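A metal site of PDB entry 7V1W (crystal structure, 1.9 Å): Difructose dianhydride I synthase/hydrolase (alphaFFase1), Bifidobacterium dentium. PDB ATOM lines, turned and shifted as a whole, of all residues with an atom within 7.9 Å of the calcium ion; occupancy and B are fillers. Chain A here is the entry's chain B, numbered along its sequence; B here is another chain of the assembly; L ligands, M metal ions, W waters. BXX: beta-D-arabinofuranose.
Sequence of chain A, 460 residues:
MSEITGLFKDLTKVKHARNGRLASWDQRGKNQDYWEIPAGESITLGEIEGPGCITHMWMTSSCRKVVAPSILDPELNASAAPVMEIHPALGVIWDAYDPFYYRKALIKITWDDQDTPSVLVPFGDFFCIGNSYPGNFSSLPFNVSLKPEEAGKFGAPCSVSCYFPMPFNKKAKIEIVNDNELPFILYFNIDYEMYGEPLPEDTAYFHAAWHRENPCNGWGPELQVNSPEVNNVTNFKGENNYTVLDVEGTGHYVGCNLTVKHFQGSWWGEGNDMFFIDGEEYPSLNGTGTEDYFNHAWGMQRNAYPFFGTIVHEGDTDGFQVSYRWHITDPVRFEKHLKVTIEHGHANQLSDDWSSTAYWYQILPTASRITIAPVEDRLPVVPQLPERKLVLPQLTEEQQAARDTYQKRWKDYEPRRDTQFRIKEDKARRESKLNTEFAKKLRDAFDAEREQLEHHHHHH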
ATOM      1  N   ASN A 226      -3.149   3.217  12.904  1.00  0.00           N
ATOM      2  CA  ASN A 226      -2.703   3.871  11.647  1.00  0.00           C
ATOM      3  C   ASN A 226      -3.723   3.655  10.542  1.00  0.00           C
ATOM      4  O   ASN A 226      -3.403   3.898   9.358  1.00  0.00           O
ATOM      5  CB  ASN A 226      -1.309   3.385  11.241  1.00  0.00           C
ATOM      6  CG  ASN A 226      -0.224   4.058  12.037  1.00  0.00           C
ATOM      7  OD1 ASN A 226      -0.379   5.212  12.441  1.00  0.00           O
ATOM      8  ND2 ASN A 226       0.858   3.341  12.288  1.00  0.00           N
ATOM      9  N   ASN A 231      -5.937   8.112  12.152  1.00  0.00           N
ATOM     10  CA  ASN A 231      -4.868   9.111  11.890  1.00  0.00           C
ATOM     11  C   ASN A 231      -5.443  10.504  11.618  1.00  0.00           C
ATOM     12  O   ASN A 231      -4.689  11.456  11.774  1.00  0.00           O
ATOM     13  CB  ASN A 231      -3.937   8.685  10.748  1.00  0.00           C
ATOM     14  CG  ASN A 231      -2.955   7.616  11.175  1.00  0.00           C
ATOM     15  OD1 ASN A 231      -2.673   7.421  12.367  1.00  0.00           O
ATOM     16  ND2 ASN A 231      -2.398   6.944  10.203  1.00  0.00           N
ATOM     17  N   GLY A 269       3.179   3.018  19.607  1.00  0.00           N
ATOM     18  CA  GLY A 269       4.048   4.207  19.738  1.00  0.00           C
ATOM     19  C   GLY A 269       3.814   5.354  18.751  1.00  0.00           C
ATOM     20  O   GLY A 269       4.744   6.187  18.611  1.00  0.00           O
ATOM     21  N   GLU A 270       2.618   5.509  18.185  1.00  0.00           N
ATOM     22  CA  GLU A 270       2.368   6.651  17.261  1.00  0.00           C
ATOM     23  C   GLU A 270       2.237   7.969  18.032  1.00  0.00           C
ATOM     24  O   GLU A 270       2.346   9.017  17.406  1.00  0.00           O
ATOM     25  CB  GLU A 270       1.091   6.415  16.452  1.00  0.00           C
ATOM     26  CG  GLU A 270       1.245   5.323  15.411  1.00  0.00           C
ATOM     27  CD  GLU A 270       2.200   5.642  14.274  1.00  0.00           C
ATOM     28  OE1 GLU A 270       2.470   6.854  14.017  1.00  0.00           O
ATOM     29  OE2 GLU A 270       2.700   4.662  13.646  1.00  0.00           O
ATOM     30  N   GLY A 271       2.031   7.930  19.366  1.00  0.00           N
ATOM     31  CA  GLY A 271       1.755   9.117  20.178  1.00  0.00           C
ATOM     32  C   GLY A 271       2.947  10.036  20.307  1.00  0.00           C
ATOM     33  O   GLY A 271       4.057   9.537  20.514  1.00  0.00           O
ATOM     34  N   ASN A 272       2.718  11.346  20.217  1.00  0.00           N
ATOM     35  CA  ASN A 272       3.769  12.395  20.338  1.00  0.00           C
ATOM     36  C   ASN A 272       4.015  12.721  21.827  1.00  0.00           C
ATOM     37  O   ASN A 272       3.061  12.851  22.578  1.00  0.00           O
ATOM     38  CB  ASN A 272       3.366  13.669  19.608  1.00  0.00           C
ATOM     39  CG  ASN A 272       3.096  13.512  18.116  1.00  0.00           C
ATOM     40  OD1 ASN A 272       3.290  12.445  17.523  1.00  0.00           O
ATOM     41  ND2 ASN A 272       2.624  14.578  17.490  1.00  0.00           N
ATOM     42  N   ASP A 273       5.277  12.916  22.204  1.00  0.00           N
ATOM     43  CA  ASP A 273       5.629  13.707  23.401  1.00  0.00           C
ATOM     44  C   ASP A 273       5.085  15.135  23.234  1.00  0.00           C
ATOM     45  O   ASP A 273       5.174  15.701  22.127  1.00  0.00           O
ATOM     46  CB  ASP A 273       7.130  13.720  23.669  1.00  0.00           C
ATOM     47  CG  ASP A 273       7.990  14.088  22.481  1.00  0.00           C
ATOM     48  OD1 ASP A 273       7.930  13.355  21.453  1.00  0.00           O
ATOM     49  OD2 ASP A 273       8.767  15.070  22.610  1.00  0.00           O
ATOM     50  N   MET A 274       4.595  15.703  24.322  1.00  0.00           N
ATOM     51  CA  MET A 274       4.092  17.095  24.382  1.00  0.00           C
ATOM     52  C   MET A 274       4.481  17.591  25.765  1.00  0.00           C
ATOM     53  O   MET A 274       4.026  16.974  26.781  1.00  0.00           O
ATOM     54  CB  MET A 274       2.570  17.196  24.160  1.00  0.00           C
ATOM     55  CG  MET A 274       2.116  16.803  22.777  1.00  0.00           C
ATOM     56  SD  MET A 274       0.341  17.008  22.537  1.00  0.00           S
ATOM     57  CE  MET A 274       0.050  16.225  20.960  1.00  0.00           C
ATOM     58  N   GLY A 287       6.540  16.744  19.774  1.00  0.00           N
ATOM     59  CA  GLY A 287       7.279  15.627  19.170  1.00  0.00           C
ATOM     60  C   GLY A 287       6.471  15.003  18.065  1.00  0.00           C
ATOM     61  O   GLY A 287       5.501  15.598  17.593  1.00  0.00           O
ATOM     62  N   THR A 288       6.883  13.824  17.620  1.00  0.00           N
ATOM     63  CA  THR A 288       6.373  13.225  16.380  1.00  0.00           C
ATOM     64  C   THR A 288       5.894  11.815  16.633  1.00  0.00           C
ATOM     65  O   THR A 288       5.094  11.344  15.804  1.00  0.00           O
ATOM     66  CB  THR A 288       7.457  13.325  15.321  1.00  0.00           C
ATOM     67  OG1 THR A 288       8.604  12.660  15.825  1.00  0.00           O
ATOM     68  CG2 THR A 288       7.752  14.779  15.045  1.00  0.00           C
ATOM     69  N   GLY A 289       6.390  11.141  17.681  1.00  0.00           N
ATOM     70  CA  GLY A 289       6.098   9.720  17.898  1.00  0.00           C
ATOM     71  C   GLY A 289       6.782   9.219  19.161  1.00  0.00           C
ATOM     72  O   GLY A 289       7.687   9.926  19.656  1.00  0.00           O
ATOM     73  N   THR A 290       6.410   8.070  19.682  1.00  0.00           N
ATOM     74  CA  THR A 290       6.914   7.653  21.017  1.00  0.00           C
ATOM     75  C   THR A 290       8.325   7.043  20.855  1.00  0.00           C
ATOM     76  O   THR A 290       9.241   7.430  21.601  1.00  0.00           O
ATOM     77  CB  THR A 290       5.909   6.719  21.709  1.00  0.00           C
ATOM     78  OG1 THR A 290       4.588   7.271  21.709  1.00  0.00           O
ATOM     79  CG2 THR A 290       6.295   6.402  23.130  1.00  0.00           C
ATOM     80  N   GLU A 291       8.543   6.189  19.859  1.00  0.00           N
ATOM     81  CA  GLU A 291       9.901   5.688  19.562  1.00  0.00           C
ATOM     82  C   GLU A 291      10.727   6.919  19.161  1.00  0.00           C
ATOM     83  O   GLU A 291      11.926   6.999  19.580  1.00  0.00           O
ATOM     84  CB  GLU A 291       9.903   4.526  18.549  1.00  0.00           C
ATOM     85  CG  GLU A 291       9.988   4.907  17.073  1.00  0.00           C
ATOM     86  CD  GLU A 291       8.624   5.131  16.454  1.00  0.00           C
ATOM     87  OE1 GLU A 291       7.784   5.901  17.047  1.00  0.00           O
ATOM     88  OE2 GLU A 291       8.392   4.539  15.401  1.00  0.00           O
ATOM     89  N   ASP A 292      10.101   7.896  18.487  1.00  0.00           N
ATOM     90  CA  ASP A 292      10.852   9.117  18.043  1.00  0.00           C
ATOM     91  C   ASP A 292      11.375   9.862  19.266  1.00  0.00           C
ATOM     92  O   ASP A 292      12.541  10.382  19.175  1.00  0.00           O
ATOM     93  CB  ASP A 292      10.005  10.052  17.149  1.00  0.00           C
ATOM     94  CG  ASP A 292       9.376   9.354  15.952  1.00  0.00           C
ATOM     95  OD1 ASP A 292       9.802   8.175  15.633  1.00  0.00           O
ATOM     96  OD2 ASP A 292       8.467   9.950  15.330  1.00  0.00           O
ATOM     97  N   GLU A 343       1.138  11.272  24.000  1.00  0.00           N
ATOM     98  CA  GLU A 343      -0.159  10.703  23.609  1.00  0.00           C
ATOM     99  C   GLU A 343      -0.033   9.176  23.724  1.00  0.00           C
ATOM    100  O   GLU A 343       0.983   8.590  23.230  1.00  0.00           O
ATOM    101  CB  GLU A 343      -0.577  11.058  22.183  1.00  0.00           C
ATOM    102  CG  GLU A 343      -0.469  12.518  21.789  1.00  0.00           C
ATOM    103  CD  GLU A 343      -0.751  12.682  20.301  1.00  0.00           C
ATOM    104  OE1 GLU A 343       0.128  12.296  19.463  1.00  0.00           O
ATOM    105  OE2 GLU A 343      -1.887  13.085  19.970  1.00  0.00           O
ATOM    106  N   GLY A 345      -0.840   6.232  22.158  1.00  0.00           N
ATOM    107  CA  GLY A 345      -1.232   6.086  20.757  1.00  0.00           C
ATOM    108  C   GLY A 345      -1.595   7.430  20.176  1.00  0.00           C
ATOM    109  O   GLY A 345      -1.699   8.412  20.937  1.00  0.00           O
ATOM    110  N   HIS A 346      -1.758   7.489  18.864  1.00  0.00           N
ATOM    111  CA  HIS A 346      -2.099   8.742  18.170  1.00  0.00           C
ATOM    112  C   HIS A 346      -3.356   9.306  18.830  1.00  0.00           C
ATOM    113  O   HIS A 346      -4.353   8.547  18.929  1.00  0.00           O
ATOM    114  CB  HIS A 346      -2.323   8.579  16.677  1.00  0.00           C
ATOM    115  CG  HIS A 346      -2.856   9.864  16.145  1.00  0.00           C
ATOM    116  ND1 HIS A 346      -2.138  11.057  16.346  1.00  0.00           N
ATOM    117  CD2 HIS A 346      -4.051  10.199  15.633  1.00  0.00           C
ATOM    118  CE1 HIS A 346      -2.856  12.051  15.869  1.00  0.00           C
ATOM    119  NE2 HIS A 346      -4.007  11.540  15.382  1.00  0.00           N
ATOM    120  N   ALA A 347      -3.301  10.564  19.236  1.00  0.00           N
ATOM    121  CA  ALA A 347      -4.432  11.299  19.846  1.00  0.00           C
ATOM    122  C   ALA A 347      -5.117  10.417  20.893  1.00  0.00           C
ATOM    123  O   ALA A 347      -6.354  10.480  21.002  1.00  0.00           O
ATOM    124  CB  ALA A 347      -5.423  11.700  18.783  1.00  0.00           C
ATOM    125  N   TRP B  25       6.246  18.057  13.604  1.00  0.00           N
ATOM    126  CA  TRP B  25       4.930  17.759  14.225  1.00  0.00           C
ATOM    127  C   TRP B  25       3.766  18.209  13.346  1.00  0.00           C
ATOM    128  O   TRP B  25       3.855  19.202  12.634  1.00  0.00           O
ATOM    129  CB  TRP B  25       4.817  18.286  15.668  1.00  0.00           C
ATOM    130  CG  TRP B  25       4.693  19.762  15.814  1.00  0.00           C
ATOM    131  CD1 TRP B  25       5.702  20.682  15.745  1.00  0.00           C
ATOM    132  CD2 TRP B  25       3.490  20.497  16.135  1.00  0.00           C
ATOM    133  NE1 TRP B  25       5.204  21.951  15.952  1.00  0.00           N
ATOM    134  CE2 TRP B  25       3.864  21.860  16.249  1.00  0.00           C
ATOM    135  CE3 TRP B  25       2.159  20.138  16.379  1.00  0.00           C
ATOM    136  CZ2 TRP B  25       2.939  22.865  16.548  1.00  0.00           C
ATOM    137  CZ3 TRP B  25       1.242  21.133  16.678  1.00  0.00           C
ATOM    138  CH2 TRP B  25       1.622  22.472  16.753  1.00  0.00           C
ATOM    139  N   ASP B  26       2.709  17.390  13.329  1.00  0.00           N
ATOM    140  CA  ASP B  26       1.539  17.605  12.436  1.00  0.00           C
ATOM    141  C   ASP B  26       0.724  18.799  12.976  1.00  0.00           C
ATOM    142  O   ASP B  26       0.112  18.677  14.046  1.00  0.00           O
ATOM    143  CB  ASP B  26       0.768  16.285  12.321  1.00  0.00           C
ATOM    144  CG  ASP B  26      -0.317  16.380  11.282  1.00  0.00           C
ATOM    145  OD1 ASP B  26      -0.750  17.549  11.016  1.00  0.00           O
ATOM    146  OD2 ASP B  26      -0.762  15.316  10.779  1.00  0.00           O
ATOM    147  N   LYS B  30      -2.948  16.023  13.689  1.00  0.00           N
ATOM    148  CA  LYS B  30      -3.216  14.621  13.272  1.00  0.00           C
ATOM    149  C   LYS B  30      -1.882  13.823  13.311  1.00  0.00           C
ATOM    150  O   LYS B  30      -0.933  14.281  13.974  1.00  0.00           O
ATOM    151  CB  LYS B  30      -3.868  14.649  11.894  1.00  0.00           C
ATOM    152  CG  LYS B  30      -5.190  15.392  11.840  1.00  0.00           C
ATOM    153  CD  LYS B  30      -5.763  15.549  10.455  1.00  0.00           C
ATOM    154  CE  LYS B  30      -6.932  16.505  10.450  1.00  0.00           C
ATOM    155  NZ  LYS B  30      -7.879  16.183   9.368  1.00  0.00           N
ATOM    156  N   ASN B  31      -1.804  12.692  12.615  1.00  0.00           N
ATOM    157  CA  ASN B  31      -0.675  11.736  12.744  1.00  0.00           C
ATOM    158  C   ASN B  31       0.213  11.683  11.479  1.00  0.00           C
ATOM    159  O   ASN B  31       0.816  10.633  11.234  1.00  0.00           O
ATOM    160  CB  ASN B  31      -1.168  10.339  13.135  1.00  0.00           C
ATOM    161  CG  ASN B  31      -0.053   9.528  13.754  1.00  0.00           C
ATOM    162  OD1 ASN B  31       0.788  10.088  14.467  1.00  0.00           O
ATOM    163  ND2 ASN B  31       0.039   8.259  13.392  1.00  0.00           N
ATOM    164  N   GLN B  32       0.393  12.825  10.802  1.00  0.00           N
ATOM    165  CA  GLN B  32       1.445  13.028   9.769  1.00  0.00           C
ATOM    166  C   GLN B  32       2.539  13.933  10.324  1.00  0.00           C
ATOM    167  O   GLN B  32       2.700  15.044   9.791  1.00  0.00           O
ATOM    168  CB  GLN B  32       0.850  13.628   8.509  1.00  0.00           C
ATOM    169  CG  GLN B  32       0.062  12.635   7.678  1.00  0.00           C
ATOM    170  CD  GLN B  32      -0.281  13.245   6.338  1.00  0.00           C
ATOM    171  OE1 GLN B  32       0.329  14.226   5.886  1.00  0.00           O
ATOM    172  NE2 GLN B  32      -1.307  12.679   5.745  1.00  0.00           N
ATOM    173  N   ASP B  33       3.302  13.435  11.295  1.00  0.00           N
ATOM    174  CA  ASP B  33       4.295  14.195  12.091  1.00  0.00           C
ATOM    175  C   ASP B  33       5.633  14.221  11.345  1.00  0.00           C
ATOM    176  O   ASP B  33       6.714  14.169  11.983  1.00  0.00           O
ATOM    177  CB  ASP B  33       4.393  13.590  13.493  1.00  0.00           C
ATOM    178  CG  ASP B  33       3.088  13.661  14.254  1.00  0.00           C
ATOM    179  OD1 ASP B  33       2.763  14.764  14.730  1.00  0.00           O
ATOM    180  OD2 ASP B  33       2.366  12.638  14.280  1.00  0.00           O
ATOM    181  N   TYR B  34       5.572  14.304  10.032  1.00  0.00           N
ATOM    182  CA  TYR B  34       6.710  14.345   9.095  1.00  0.00           C
ATOM    183  C   TYR B  34       6.420  15.386   8.022  1.00  0.00           C
ATOM    184  O   TYR B  34       5.242  15.721   7.796  1.00  0.00           O
ATOM    185  CB  TYR B  34       6.916  12.965   8.478  1.00  0.00           C
ATOM    186  CG  TYR B  34       5.736  12.474   7.684  1.00  0.00           C
ATOM    187  CD1 TYR B  34       5.638  12.754   6.327  1.00  0.00           C
ATOM    188  CD2 TYR B  34       4.770  11.665   8.252  1.00  0.00           C
ATOM    189  CE1 TYR B  34       4.547  12.332   5.581  1.00  0.00           C
ATOM    190  CE2 TYR B  34       3.671  11.237   7.504  1.00  0.00           C
ATOM    191  CZ  TYR B  34       3.589  11.540   6.161  1.00  0.00           C
ATOM    192  OH  TYR B  34       2.532  11.121   5.386  1.00  0.00           O
ATOM    193  N   TYR B 187      11.151  13.173   9.261  1.00  0.00           N
ATOM    194  CA  TYR B 187      10.742  13.369  10.661  1.00  0.00           C
ATOM    195  C   TYR B 187      11.925  14.075  11.319  1.00  0.00           C
ATOM    196  O   TYR B 187      13.055  13.634  11.052  1.00  0.00           O
ATOM    197  CB  TYR B 187      10.486  12.025  11.363  1.00  0.00           C
ATOM    198  CG  TYR B 187       9.196  11.307  11.063  1.00  0.00           C
ATOM    199  CD1 TYR B 187       9.080  10.441   9.981  1.00  0.00           C
ATOM    200  CD2 TYR B 187       8.122  11.393  11.924  1.00  0.00           C
ATOM    201  CE1 TYR B 187       7.887   9.752   9.732  1.00  0.00           C
ATOM    202  CE2 TYR B 187       6.936  10.702  11.698  1.00  0.00           C
ATOM    203  CZ  TYR B 187       6.804   9.897  10.580  1.00  0.00           C
ATOM    204  OH  TYR B 187       5.616   9.231  10.380  1.00  0.00           O
HETATM  205  O2  BXX L   1       5.484   5.918  15.761  1.00  0.00           O
HETATM  206  C2  BXX L   1       5.724   6.228  14.343  1.00  0.00           C
HETATM  207  C1  BXX L   1       6.089   5.096  13.359  1.00  0.00           C
HETATM  208  O4  BXX L   1       7.169   5.586  12.514  1.00  0.00           O
HETATM  209  C3  BXX L   1       6.840   7.248  14.135  1.00  0.00           C
HETATM  210  O3  BXX L   1       6.504   8.644  14.348  1.00  0.00           O
HETATM  211  C4  BXX L   1       7.387   6.968  12.715  1.00  0.00           C
HETATM  212  C5  BXX L   1       8.837   7.330  12.439  1.00  0.00           C
HETATM  213  O5  BXX L   1       9.780   6.757  13.362  1.00  0.00           O
HETATM  214  O1  BXX L   1       6.481   3.797  13.938  1.00  0.00           O
HETATM  215 CA    CA M   1       2.523  10.891  15.875  1.00  0.00          CA
HETATM  216  O   HOH W   1       3.717   9.156  14.509  1.00  0.00           O
HETATM  217  O   HOH W   2       0.453  11.959  16.932  1.00  0.00           O
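Of the 26 residues printed, 5 come within 4 Å of the calcium ion.
Water W2 lies within hydrogen-bond range of OE1 of Glu 343 (2.6 Å), ND1 of His 346 (2.8 Å) and ND2 of Asn 272 (3.4 Å). Water W1 bridges OE1 of Glu 270 and O3 of the ligand.
The backbone carbonyl oxygen of Thr 288 sits close to an oxygen (O3) of the ligand, 3.4 Å away. An oxygen (O2) of the ligand sits at hydrogen-bond distance from the backbone carbonyl oxygen (O) of Gly 269 (3.0 Å). The side-chain carboxylate (OD2) of Asp 292 lies within hydrogen-bond range of an oxygen (O3) of the ligand, at 2.6 Å. The side-chain carboxylate (OE2) of Glu 291 sits at hydrogen-bond distance from an oxygen (O1) of the ligand (2.5 Å).
The side-chain carboxylate of Asp 33 of chain B sits at hydrogen-bond distance from the backbone NH of Asp 26 of chain B, 3.0 Å away. The backbone NH (N) of Asn 31 of chain B sits at hydrogen-bond distance from the side-chain carboxylate (OD2) of Asp 26 of chain B (3.4 Å). The side-chain amide nitrogen (ND2) of Asn 31 of chain B sits at hydrogen-bond distance from the side-chain amide oxygen (OD1) of Asn 226 (3.2 Å). The side-chain amide oxygen of Asn 272 lies close to the backbone NH of Gly 289. The backbone NH of Asn 272 is in hydrogen-bond range of the side-chain carboxylate of Glu 343 (2.9 Å). ND2 of Asn 272 is in hydrogen-bond range of O of Gly 287 (3.1 Å). The side-chain amide nitrogen of Asn 226 sits at hydrogen-bond distance from the side-chain carboxylate of Glu 270 (2.6 Å). The side-chain hydroxyl (OG1) of Thr 288 sits at hydrogen-bond distance from the side-chain carboxylate (OD2) of Asp 292 (2.8 Å).
The calcium ion is bound by the side-chain carboxylate (OD2) of Asp 33 of chain B (2.4 Å), the side-chain amide oxygen (OD1) of Asn 31 of chain B (2.4 Å), the side-chain amide oxygen (OD1) of Asn 272 (2.4 Å), the backbone carbonyl oxygen (O) of Glu 270 (2.4 Å), water W1 (2.5 Å), water W2 (2.6 Å) and the backbone carbonyl oxygen (O) of Thr 288 (2.6 Å).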
